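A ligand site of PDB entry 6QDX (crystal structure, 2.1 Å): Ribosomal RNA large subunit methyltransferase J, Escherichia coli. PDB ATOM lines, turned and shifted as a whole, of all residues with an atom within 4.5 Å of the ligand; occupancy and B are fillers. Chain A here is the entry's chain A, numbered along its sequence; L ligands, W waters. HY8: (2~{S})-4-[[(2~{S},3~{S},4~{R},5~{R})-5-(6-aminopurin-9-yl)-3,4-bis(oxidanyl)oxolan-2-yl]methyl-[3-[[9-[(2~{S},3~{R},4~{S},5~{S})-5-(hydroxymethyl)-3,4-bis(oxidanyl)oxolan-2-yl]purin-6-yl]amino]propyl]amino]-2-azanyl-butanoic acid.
The side-chain carboxylate (OD2) of Asp 18 lies within hydrogen-bond range of an oxygen (O9) of the ligand (2.5 Å).
The backbone carbonyl oxygen (O) of His 45 is in hydrogen-bond range of a nitrogen (N7) of the ligand.
The side-chain carboxylate of Asp 167 lies within salt-bridge range of a nitrogen (N7) of the ligand, 2.8 Å away.
The backbone carbonyl oxygen (O) of Pro 169 is in hydrogen-bond range of an oxygen (O4) of the ligand, 2.9 Å away.
The side-chain amino group of Lys 21 lies within salt-bridge range of an oxygen (O6) of the ligand, 3.2 Å away.
O5 of the ligand is in hydrogen-bond range of N of Ser 103.
OG of Ser 103 lies close to O6 of the ligand (3.1 Å).
NE2 of His 22 lies within hydrogen-bond range of O6 of the ligand (3.1 Å).
The side-chain carboxylate (OD1) of Asp 43 lies within salt-bridge range of a nitrogen (N7) of the ligand, at 3.5 Å.
OD1 of Asp 18 is in salt-bridge range of NZ of Lys 21, at 3.4 Å.
The backbone carbonyl oxygen (O) of Asp 18 lies close to a ring nitrogen (ND1) of His 22 (3.3 Å).
OD2 of Asp 18 is in hydrogen-bond range of N of Gly 14 (2.8 Å).
The backbone NH (N) of Asp 18 lies within hydrogen-bond range of the side-chain amide oxygen (OD1) of Asn 15.
The side-chain carboxylate (OD2) of Asp 167 is in salt-bridge range of the side-chain amino group (NZ) of Lys 21 (2.6 Å).
The side-chain carboxylate (OD2) of Asp 43 sits at hydrogen-bond distance from the side-chain hydroxyl (OG) of Ser 103, at 2.4 Å.
The backbone NH of His 12 lies close to the side-chain hydroxyl of Ser 10.
The backbone NH (N) of Ala 13 sits at hydrogen-bond distance from the side-chain hydroxyl (OG) of Ser 10 (3.2 Å).
His 12 touches the ligand (CD2 to C27, 3.4 Å).
Ala 13 touches the ligand (CA to O9, 3.5 Å).
O of Ala 46 touches C16 of the ligand (3.2 Å).
Gly 47 touches the ligand.
Gly 102 touches the ligand (CA to O5, 3.6 Å).
Tyr 170 touches the ligand (O to O4, 3.7 Å).
Glu 171 touches the ligand.
Val 202 touches the ligand (CG2 to O3, 3.7 Å).
Met 238 touches the ligand (CE to O2, 3.5 Å).
Hydrophobic or aromatic side chains within 4 Å of the ligand: His 12, Ala 13, His 22, Pro 169, Val 202 and Met 238.
The nearest printed residue that does not touch the ligand is Ser 10 (4.05 Å).
Water W3 bridges O9 of the ligand (2.6 Å) and OD2 of Asp 18 (3.1 Å).
Water W1 bridges OG of Ser 10 (2.6 Å) and N10 of the ligand (2.8 Å).
Water W2 lies within hydrogen-bond range of O2 of the ligand (2.9 Å), ND2 of Asn 15 (2.9 Å) and ND1 of His 12 (3.4 Å).
Water W4 lies within hydrogen-bond range of the backbone carbonyl oxygen of Ala 46, an oxygen (O5) of the ligand and the side-chain hydroxyl of Tyr 51.
Water W5 lies within hydrogen-bond range of ND2 of Asn 15 and OD1 of Asp 18.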
ATOM      1  N   SER A  10      18.801 -19.762 -17.160  1.00  0.00           N
ATOM      2  CA  SER A  10      17.949 -20.951 -17.160  1.00  0.00           C
ATOM      3  C   SER A  10      16.516 -20.550 -17.422  1.00  0.00           C
ATOM      4  O   SER A  10      15.982 -19.682 -16.717  1.00  0.00           O
ATOM      5  CB  SER A  10      18.055 -21.710 -15.838  1.00  0.00           C
ATOM      6  OG  SER A  10      17.194 -22.837 -15.857  1.00  0.00           O
ATOM      7  N   HIS A  12      13.963 -22.620 -17.016  1.00  0.00           N
ATOM      8  CA  HIS A  12      13.129 -23.322 -16.056  1.00  0.00           C
ATOM      9  C   HIS A  12      13.356 -22.886 -14.618  1.00  0.00           C
ATOM     10  O   HIS A  12      12.510 -23.183 -13.777  1.00  0.00           O
ATOM     11  CB  HIS A  12      13.344 -24.831 -16.136  1.00  0.00           C
ATOM     12  CG  HIS A  12      13.234 -25.378 -17.527  1.00  0.00           C
ATOM     13  ND1 HIS A  12      12.110 -26.052 -17.976  1.00  0.00           N
ATOM     14  CD2 HIS A  12      14.099 -25.372 -18.559  1.00  0.00           C
ATOM     15  CE1 HIS A  12      12.296 -26.427 -19.226  1.00  0.00           C
ATOM     16  NE2 HIS A  12      13.499 -26.023 -19.611  1.00  0.00           N
ATOM     17  N   ALA A  13      14.462 -22.198 -14.298  1.00  0.00           N
ATOM     18  CA  ALA A  13      14.776 -21.904 -12.910  1.00  0.00           C
ATOM     19  C   ALA A  13      13.679 -21.061 -12.244  1.00  0.00           C
ATOM     20  O   ALA A  13      13.140 -20.128 -12.848  1.00  0.00           O
ATOM     21  CB  ALA A  13      16.126 -21.209 -12.790  1.00  0.00           C
ATOM     22  N   GLY A  14      13.373 -21.402 -10.999  1.00  0.00           N
ATOM     23  CA  GLY A  14      12.356 -20.729 -10.220  1.00  0.00           C
ATOM     24  C   GLY A  14      10.925 -21.049 -10.598  1.00  0.00           C
ATOM     25  O   GLY A  14      10.022 -20.297 -10.234  1.00  0.00           O
ATOM     26  N   ASN A  15      10.707 -22.147 -11.332  1.00  0.00           N
ATOM     27  CA  ASN A  15       9.375 -22.599 -11.701  1.00  0.00           C
ATOM     28  C   ASN A  15       8.648 -23.139 -10.464  1.00  0.00           C
ATOM     29  O   ASN A  15       9.214 -23.225  -9.368  1.00  0.00           O
ATOM     30  CB  ASN A  15       9.460 -23.660 -12.809  1.00  0.00           C
ATOM     31  CG  ASN A  15      10.182 -24.920 -12.343  1.00  0.00           C
ATOM     32  OD1 ASN A  15      10.747 -24.948 -11.262  1.00  0.00           O
ATOM     33  ND2 ASN A  15      10.162 -25.961 -13.159  1.00  0.00           N
ATOM     34  N   ASP A  18      10.521 -25.646  -8.481  1.00  0.00           N
ATOM     35  CA  ASP A  18      11.540 -25.030  -7.637  1.00  0.00           C
ATOM     36  C   ASP A  18      10.938 -24.422  -6.366  1.00  0.00           C
ATOM     37  O   ASP A  18      11.521 -24.548  -5.270  1.00  0.00           O
ATOM     38  CB  ASP A  18      12.300 -23.974  -8.456  1.00  0.00           C
ATOM     39  CG  ASP A  18      13.438 -24.575  -9.263  1.00  0.00           C
ATOM     40  OD1 ASP A  18      13.629 -25.818  -9.196  1.00  0.00           O
ATOM     41  OD2 ASP A  18      14.163 -23.818  -9.935  1.00  0.00           O
ATOM     42  N   LYS A  21      10.132 -27.445  -4.038  1.00  0.00           N
ATOM     43  CA  LYS A  21      11.323 -28.170  -3.599  1.00  0.00           C
ATOM     44  C   LYS A  21      12.127 -27.348  -2.599  1.00  0.00           C
ATOM     45  O   LYS A  21      12.552 -27.829  -1.539  1.00  0.00           O
ATOM     46  CB  LYS A  21      12.179 -28.532  -4.818  1.00  0.00           C
ATOM     47  CG  LYS A  21      13.507 -29.159  -4.490  1.00  0.00           C
ATOM     48  CD  LYS A  21      14.538 -28.870  -5.555  1.00  0.00           C
ATOM     49  CE  LYS A  21      14.046 -29.265  -6.926  1.00  0.00           C
ATOM     50  NZ  LYS A  21      14.948 -28.757  -7.975  1.00  0.00           N
ATOM     51  N   HIS A  22      12.333 -26.081  -2.920  1.00  0.00           N
ATOM     52  CA  HIS A  22      13.152 -25.223  -2.092  1.00  0.00           C
ATOM     53  C   HIS A  22      12.421 -24.776  -0.845  1.00  0.00           C
ATOM     54  O   HIS A  22      13.052 -24.599   0.208  1.00  0.00           O
ATOM     55  CB  HIS A  22      13.649 -24.061  -2.935  1.00  0.00           C
ATOM     56  CG  HIS A  22      14.630 -24.488  -3.975  1.00  0.00           C
ATOM     57  ND1 HIS A  22      14.761 -23.867  -5.195  1.00  0.00           N
ATOM     58  CD2 HIS A  22      15.516 -25.519  -3.978  1.00  0.00           C
ATOM     59  CE1 HIS A  22      15.699 -24.481  -5.903  1.00  0.00           C
ATOM     60  NE2 HIS A  22      16.171 -25.498  -5.191  1.00  0.00           N
ATOM     61  N   ASP A  43      23.885 -32.891  -1.472  1.00  0.00           N
ATOM     62  CA  ASP A  43      23.142 -32.504  -2.700  1.00  0.00           C
ATOM     63  C   ASP A  43      23.664 -33.402  -3.822  1.00  0.00           C
ATOM     64  O   ASP A  43      24.737 -33.139  -4.386  1.00  0.00           O
ATOM     65  CB  ASP A  43      23.332 -31.012  -3.010  1.00  0.00           C
ATOM     66  CG  ASP A  43      22.172 -30.377  -3.812  1.00  0.00           C
ATOM     67  OD1 ASP A  43      21.566 -31.062  -4.656  1.00  0.00           O
ATOM     68  OD2 ASP A  43      21.861 -29.185  -3.578  1.00  0.00           O
ATOM     69  N   HIS A  45      22.775 -33.909  -6.882  1.00  0.00           N
ATOM     70  CA  HIS A  45      22.750 -33.303  -8.224  1.00  0.00           C
ATOM     71  C   HIS A  45      22.561 -31.798  -8.023  1.00  0.00           C
ATOM     72  O   HIS A  45      21.435 -31.319  -7.957  1.00  0.00           O
ATOM     73  CB  HIS A  45      21.633 -33.908  -9.079  1.00  0.00           C
ATOM     74  CG  HIS A  45      21.737 -35.406  -9.219  1.00  0.00           C
ATOM     75  ND1 HIS A  45      21.293 -36.266  -8.252  1.00  0.00           N
ATOM     76  CD2 HIS A  45      22.234 -36.178 -10.208  1.00  0.00           C
ATOM     77  CE1 HIS A  45      21.501 -37.515  -8.637  1.00  0.00           C
ATOM     78  NE2 HIS A  45      22.078 -37.485  -9.830  1.00  0.00           N
ATOM     79  N   ALA A  46      23.677 -31.065  -7.931  1.00  0.00           N
ATOM     80  CA  ALA A  46      23.649 -29.716  -7.387  1.00  0.00           C
ATOM     81  C   ALA A  46      23.451 -28.621  -8.443  1.00  0.00           C
ATOM     82  O   ALA A  46      23.126 -27.496  -8.068  1.00  0.00           O
ATOM     83  CB  ALA A  46      24.921 -29.423  -6.596  1.00  0.00           C
ATOM     84  N   GLY A  47      23.632 -28.914  -9.722  1.00  0.00           N
ATOM     85  CA  GLY A  47      23.439 -27.882 -10.728  1.00  0.00           C
ATOM     86  C   GLY A  47      24.513 -26.800 -10.645  1.00  0.00           C
ATOM     87  O   GLY A  47      25.632 -27.026 -10.172  1.00  0.00           O
ATOM     88  N   TYR A  51      21.036 -18.897 -10.831  1.00  0.00           N
ATOM     89  CA  TYR A  51      20.540 -18.798 -12.193  1.00  0.00           C
ATOM     90  C   TYR A  51      20.156 -17.365 -12.500  1.00  0.00           C
ATOM     91  O   TYR A  51      19.467 -16.716 -11.696  1.00  0.00           O
ATOM     92  CB  TYR A  51      19.365 -19.743 -12.406  1.00  0.00           C
ATOM     93  CG  TYR A  51      19.781 -21.159 -12.174  1.00  0.00           C
ATOM     94  CD1 TYR A  51      20.498 -21.842 -13.149  1.00  0.00           C
ATOM     95  CD2 TYR A  51      19.553 -21.782 -10.953  1.00  0.00           C
ATOM     96  CE1 TYR A  51      20.920 -23.125 -12.945  1.00  0.00           C
ATOM     97  CE2 TYR A  51      19.983 -23.072 -10.723  1.00  0.00           C
ATOM     98  CZ  TYR A  51      20.675 -23.740 -11.732  1.00  0.00           C
ATOM     99  OH  TYR A  51      21.113 -25.041 -11.531  1.00  0.00           O
ATOM    100  N   GLY A 102      19.864 -21.724  -6.597  1.00  0.00           N
ATOM    101  CA  GLY A 102      19.690 -23.162  -6.601  1.00  0.00           C
ATOM    102  C   GLY A 102      19.777 -23.736  -5.201  1.00  0.00           C
ATOM    103  O   GLY A 102      20.126 -23.041  -4.241  1.00  0.00           O
ATOM    104  N   SER A 103      19.443 -25.011  -5.078  1.00  0.00           N
ATOM    105  CA  SER A 103      19.510 -25.663  -3.770  1.00  0.00           C
ATOM    106  C   SER A 103      20.853 -25.544  -3.056  1.00  0.00           C
ATOM    107  O   SER A 103      20.855 -25.446  -1.826  1.00  0.00           O
ATOM    108  CB  SER A 103      19.127 -27.149  -3.894  1.00  0.00           C
ATOM    109  OG  SER A 103      20.076 -27.909  -4.621  1.00  0.00           O
ATOM    110  N   PRO A 104      22.011 -25.534  -3.731  1.00  0.00           N
ATOM    111  CA  PRO A 104      23.277 -25.400  -2.965  1.00  0.00           C
ATOM    112  C   PRO A 104      23.401 -24.057  -2.288  1.00  0.00           C
ATOM    113  O   PRO A 104      24.038 -23.973  -1.215  1.00  0.00           O
ATOM    114  CB  PRO A 104      24.377 -25.590  -4.034  1.00  0.00           C
ATOM    115  CG  PRO A 104      23.717 -26.283  -5.154  1.00  0.00           C
ATOM    116  CD  PRO A 104      22.280 -25.781  -5.150  1.00  0.00           C
ATOM    117  N   LEU A 165      19.435 -34.293  -0.270  1.00  0.00           N
ATOM    118  CA  LEU A 165      18.522 -33.980  -1.370  1.00  0.00           C
ATOM    119  C   LEU A 165      18.939 -34.754  -2.602  1.00  0.00           C
ATOM    120  O   LEU A 165      20.085 -34.669  -3.045  1.00  0.00           O
ATOM    121  CB  LEU A 165      18.496 -32.483  -1.677  1.00  0.00           C
ATOM    122  CG  LEU A 165      17.522 -31.968  -2.772  1.00  0.00           C
ATOM    123  CD1 LEU A 165      16.081 -31.984  -2.299  1.00  0.00           C
ATOM    124  CD2 LEU A 165      17.880 -30.558  -3.189  1.00  0.00           C
ATOM    125  N   ASP A 167      17.989 -35.112  -6.376  1.00  0.00           N
ATOM    126  CA  ASP A 167      17.293 -34.222  -7.309  1.00  0.00           C
ATOM    127  C   ASP A 167      17.814 -34.403  -8.731  1.00  0.00           C
ATOM    128  O   ASP A 167      18.287 -33.445  -9.352  1.00  0.00           O
ATOM    129  CB  ASP A 167      17.425 -32.779  -6.853  1.00  0.00           C
ATOM    130  CG  ASP A 167      16.502 -31.838  -7.583  1.00  0.00           C
ATOM    131  OD1 ASP A 167      15.600 -32.320  -8.330  1.00  0.00           O
ATOM    132  OD2 ASP A 167      16.709 -30.621  -7.419  1.00  0.00           O
ATOM    133  N   PRO A 169      17.944 -35.177 -12.923  1.00  0.00           N
ATOM    134  CA  PRO A 169      17.221 -34.497 -14.018  1.00  0.00           C
ATOM    135  C   PRO A 169      16.000 -35.244 -14.516  1.00  0.00           C
ATOM    136  O   PRO A 169      15.131 -34.616 -15.124  1.00  0.00           O
ATOM    137  CB  PRO A 169      18.276 -34.399 -15.126  1.00  0.00           C
ATOM    138  CG  PRO A 169      19.609 -34.665 -14.458  1.00  0.00           C
ATOM    139  CD  PRO A 169      19.298 -35.583 -13.319  1.00  0.00           C
ATOM    140  N   TYR A 170      15.944 -36.562 -14.311  1.00  0.00           N
ATOM    141  CA  TYR A 170      14.916 -37.437 -14.891  1.00  0.00           C
ATOM    142  C   TYR A 170      14.859 -37.311 -16.412  1.00  0.00           C
ATOM    143  O   TYR A 170      13.804 -37.503 -17.016  1.00  0.00           O
ATOM    144  CB  TYR A 170      13.529 -37.199 -14.268  1.00  0.00           C
ATOM    145  CG  TYR A 170      13.462 -37.550 -12.797  1.00  0.00           C
ATOM    146  CD1 TYR A 170      13.742 -36.596 -11.829  1.00  0.00           C
ATOM    147  CD2 TYR A 170      13.131 -38.843 -12.365  1.00  0.00           C
ATOM    148  CE1 TYR A 170      13.668 -36.898 -10.474  1.00  0.00           C
ATOM    149  CE2 TYR A 170      13.070 -39.149 -11.015  1.00  0.00           C
ATOM    150  CZ  TYR A 170      13.341 -38.166 -10.075  1.00  0.00           C
ATOM    151  OH  TYR A 170      13.296 -38.435  -8.720  1.00  0.00           O
ATOM    152  N   GLU A 171      15.988 -36.988 -17.032  1.00  0.00           N
ATOM    153  CA  GLU A 171      16.087 -37.070 -18.482  1.00  0.00           C
ATOM    154  C   GLU A 171      16.150 -38.520 -18.949  1.00  0.00           C
ATOM    155  O   GLU A 171      15.514 -38.890 -19.937  1.00  0.00           O
ATOM    156  CB  GLU A 171      17.308 -36.290 -18.949  1.00  0.00           C
ATOM    157  CG  GLU A 171      17.071 -35.423 -20.160  1.00  0.00           C
ATOM    158  CD  GLU A 171      18.359 -34.818 -20.696  1.00  0.00           C
ATOM    159  OE1 GLU A 171      19.387 -35.531 -20.745  1.00  0.00           O
ATOM    160  OE2 GLU A 171      18.337 -33.628 -21.101  1.00  0.00           O
ATOM    161  N   PRO A 200       9.271 -35.248 -10.795  1.00  0.00           N
ATOM    162  CA  PRO A 200       8.264 -34.554 -11.632  1.00  0.00           C
ATOM    163  C   PRO A 200       7.120 -35.474 -12.063  1.00  0.00           C
ATOM    164  O   PRO A 200       7.317 -36.686 -12.181  1.00  0.00           O
ATOM    165  CB  PRO A 200       9.088 -34.123 -12.853  1.00  0.00           C
ATOM    166  CG  PRO A 200      10.125 -35.266 -13.012  1.00  0.00           C
ATOM    167  CD  PRO A 200      10.323 -35.878 -11.605  1.00  0.00           C
ATOM    168  N   VAL A 202       5.279 -36.298 -15.257  1.00  0.00           N
ATOM    169  CA  VAL A 202       5.076 -36.141 -16.691  1.00  0.00           C
ATOM    170  C   VAL A 202       4.022 -37.157 -17.108  1.00  0.00           C
ATOM    171  O   VAL A 202       2.927 -36.791 -17.559  1.00  0.00           O
ATOM    172  CB  VAL A 202       6.370 -36.317 -17.490  1.00  0.00           C
ATOM    173  CG1 VAL A 202       6.070 -36.277 -18.969  1.00  0.00           C
ATOM    174  CG2 VAL A 202       7.390 -35.230 -17.081  1.00  0.00           C
ATOM    175  N   MET A 238       5.550 -31.907 -17.899  1.00  0.00           N
ATOM    176  CA  MET A 238       5.440 -31.865 -16.440  1.00  0.00           C
ATOM    177  C   MET A 238       4.230 -31.027 -16.053  1.00  0.00           C
ATOM    178  O   MET A 238       4.213 -29.809 -16.260  1.00  0.00           O
ATOM    179  CB  MET A 238       6.686 -31.301 -15.799  1.00  0.00           C
ATOM    180  CG  MET A 238       6.597 -31.286 -14.285  1.00  0.00           C
ATOM    181  SD  MET A 238       8.061 -30.673 -13.465  1.00  0.00           S
ATOM    182  CE  MET A 238       8.046 -28.950 -13.945  1.00  0.00           C
HETATM  183  C4  HY8 L   1      13.113 -31.841 -15.853  1.00  0.00           C
HETATM  184  C14 HY8 L   1      17.724 -29.086 -11.385  1.00  0.00           C
HETATM  185  C5  HY8 L   1      10.132 -30.262 -16.839  1.00  0.00           C
HETATM  186  C6  HY8 L   1      15.673 -31.616 -16.352  1.00  0.00           C
HETATM  187  C11 HY8 L   1      19.413 -30.534 -14.093  1.00  0.00           C
HETATM  188  C7  HY8 L   1      16.762 -31.124 -15.633  1.00  0.00           C
HETATM  189  C8  HY8 L   1      14.953 -30.918 -14.428  1.00  0.00           C
HETATM  190  C9  HY8 L   1      17.099 -32.147 -18.110  1.00  0.00           C
HETATM  191  C10 HY8 L   1      18.056 -31.161 -16.234  1.00  0.00           C
HETATM  192  C12 HY8 L   1      19.565 -29.062 -13.675  1.00  0.00           C
HETATM  193  C13 HY8 L   1      20.110 -28.917 -12.242  1.00  0.00           C
HETATM  194  N1  HY8 L   1      14.576 -31.491 -15.562  1.00  0.00           N
HETATM  195  N2  HY8 L   1      16.264 -30.683 -14.448  1.00  0.00           N
HETATM  196  C3  HY8 L   1      12.577 -33.011 -15.782  1.00  0.00           C
HETATM  197  N3  HY8 L   1      15.874 -32.120 -17.588  1.00  0.00           N
HETATM  198  C1  HY8 L   1      11.218 -31.272 -16.296  1.00  0.00           C
HETATM  199  C15 HY8 L   1      19.546 -29.421  -9.928  1.00  0.00           C
HETATM  200  C16 HY8 L   1      20.238 -28.447  -8.967  1.00  0.00           C
HETATM  201  C17 HY8 L   1      19.820 -28.593  -7.489  1.00  0.00           C
HETATM  202  C18 HY8 L   1      18.728 -27.564  -7.281  1.00  0.00           C
HETATM  203  C19 HY8 L   1      16.766 -27.971 -11.988  1.00  0.00           C
HETATM  204  C2  HY8 L   1      10.998 -32.530 -16.090  1.00  0.00           C
HETATM  205  C20 HY8 L   1      15.804 -27.413 -11.265  1.00  0.00           C
HETATM  206  C21 HY8 L   1      15.460 -26.003 -12.144  1.00  0.00           C
HETATM  207  C22 HY8 L   1      16.154 -26.099 -13.178  1.00  0.00           C
HETATM  208  C23 HY8 L   1      15.931 -27.191 -15.436  1.00  0.00           C
HETATM  209  C24 HY8 L   1      14.961 -27.953 -16.074  1.00  0.00           C
HETATM  210  C25 HY8 L   1      14.249 -27.487 -14.076  1.00  0.00           C
HETATM  211  C26 HY8 L   1      17.271 -27.284 -17.326  1.00  0.00           C
HETATM  212  C27 HY8 L   1      15.225 -28.363 -17.398  1.00  0.00           C
HETATM  213  N10 HY8 L   1      17.059 -26.875 -16.089  1.00  0.00           N
HETATM  214  N11 HY8 L   1      16.374 -28.010 -17.978  1.00  0.00           N
HETATM  215  N12 HY8 L   1      14.268 -29.153 -18.116  1.00  0.00           N
HETATM  216  N4  HY8 L   1      18.168 -31.683 -17.452  1.00  0.00           N
HETATM  217  N5  HY8 L   1      19.283 -30.647 -15.554  1.00  0.00           N
HETATM  218  N6  HY8 L   1      19.119 -28.656 -11.151  1.00  0.00           N
HETATM  219  N7  HY8 L   1      19.379 -29.928  -7.124  1.00  0.00           N
HETATM  220  N8  HY8 L   1      15.447 -26.916 -14.201  1.00  0.00           N
HETATM  221  N9  HY8 L   1      13.942 -28.112 -15.209  1.00  0.00           N
HETATM  222  O1  HY8 L   1      12.496 -31.269 -17.157  1.00  0.00           O
HETATM  223  O2  HY8 L   1      10.652 -29.024 -16.342  1.00  0.00           O
HETATM  224  O3  HY8 L   1      10.509 -33.247 -17.264  1.00  0.00           O
HETATM  225  O4  HY8 L   1      12.957 -33.953 -16.855  1.00  0.00           O
HETATM  226  O5  HY8 L   1      18.898 -26.447  -7.860  1.00  0.00           O
HETATM  227  O6  HY8 L   1      17.710 -27.828  -6.551  1.00  0.00           O
HETATM  228  O7  HY8 L   1      17.509 -26.825 -12.678  1.00  0.00           O
HETATM  229  O8  HY8 L   1      16.099 -27.006  -9.926  1.00  0.00           O
HETATM  230  O9  HY8 L   1      15.886 -24.861 -11.343  1.00  0.00           O
HETATM  231  O   HOH W   1      18.916 -24.759 -15.664  1.00  0.00           O
HETATM  232  O   HOH W   2       9.415 -26.474 -15.958  1.00  0.00           O
HETATM  233  O   HOH W   3      17.119 -24.366  -9.127  1.00  0.00           O
HETATM  234  O   HOH W   4      21.567 -25.532  -8.641  1.00  0.00           O
HETATM  235  O   HOH W   5      12.452 -27.671 -11.713  1.00  0.00           O
HETATM  236  O   HOH W   6      13.825 -29.835 -11.187  1.00  0.00           O
HETATM  237  O   HOH W   7      19.121 -32.021 -11.355  1.00  0.00           O
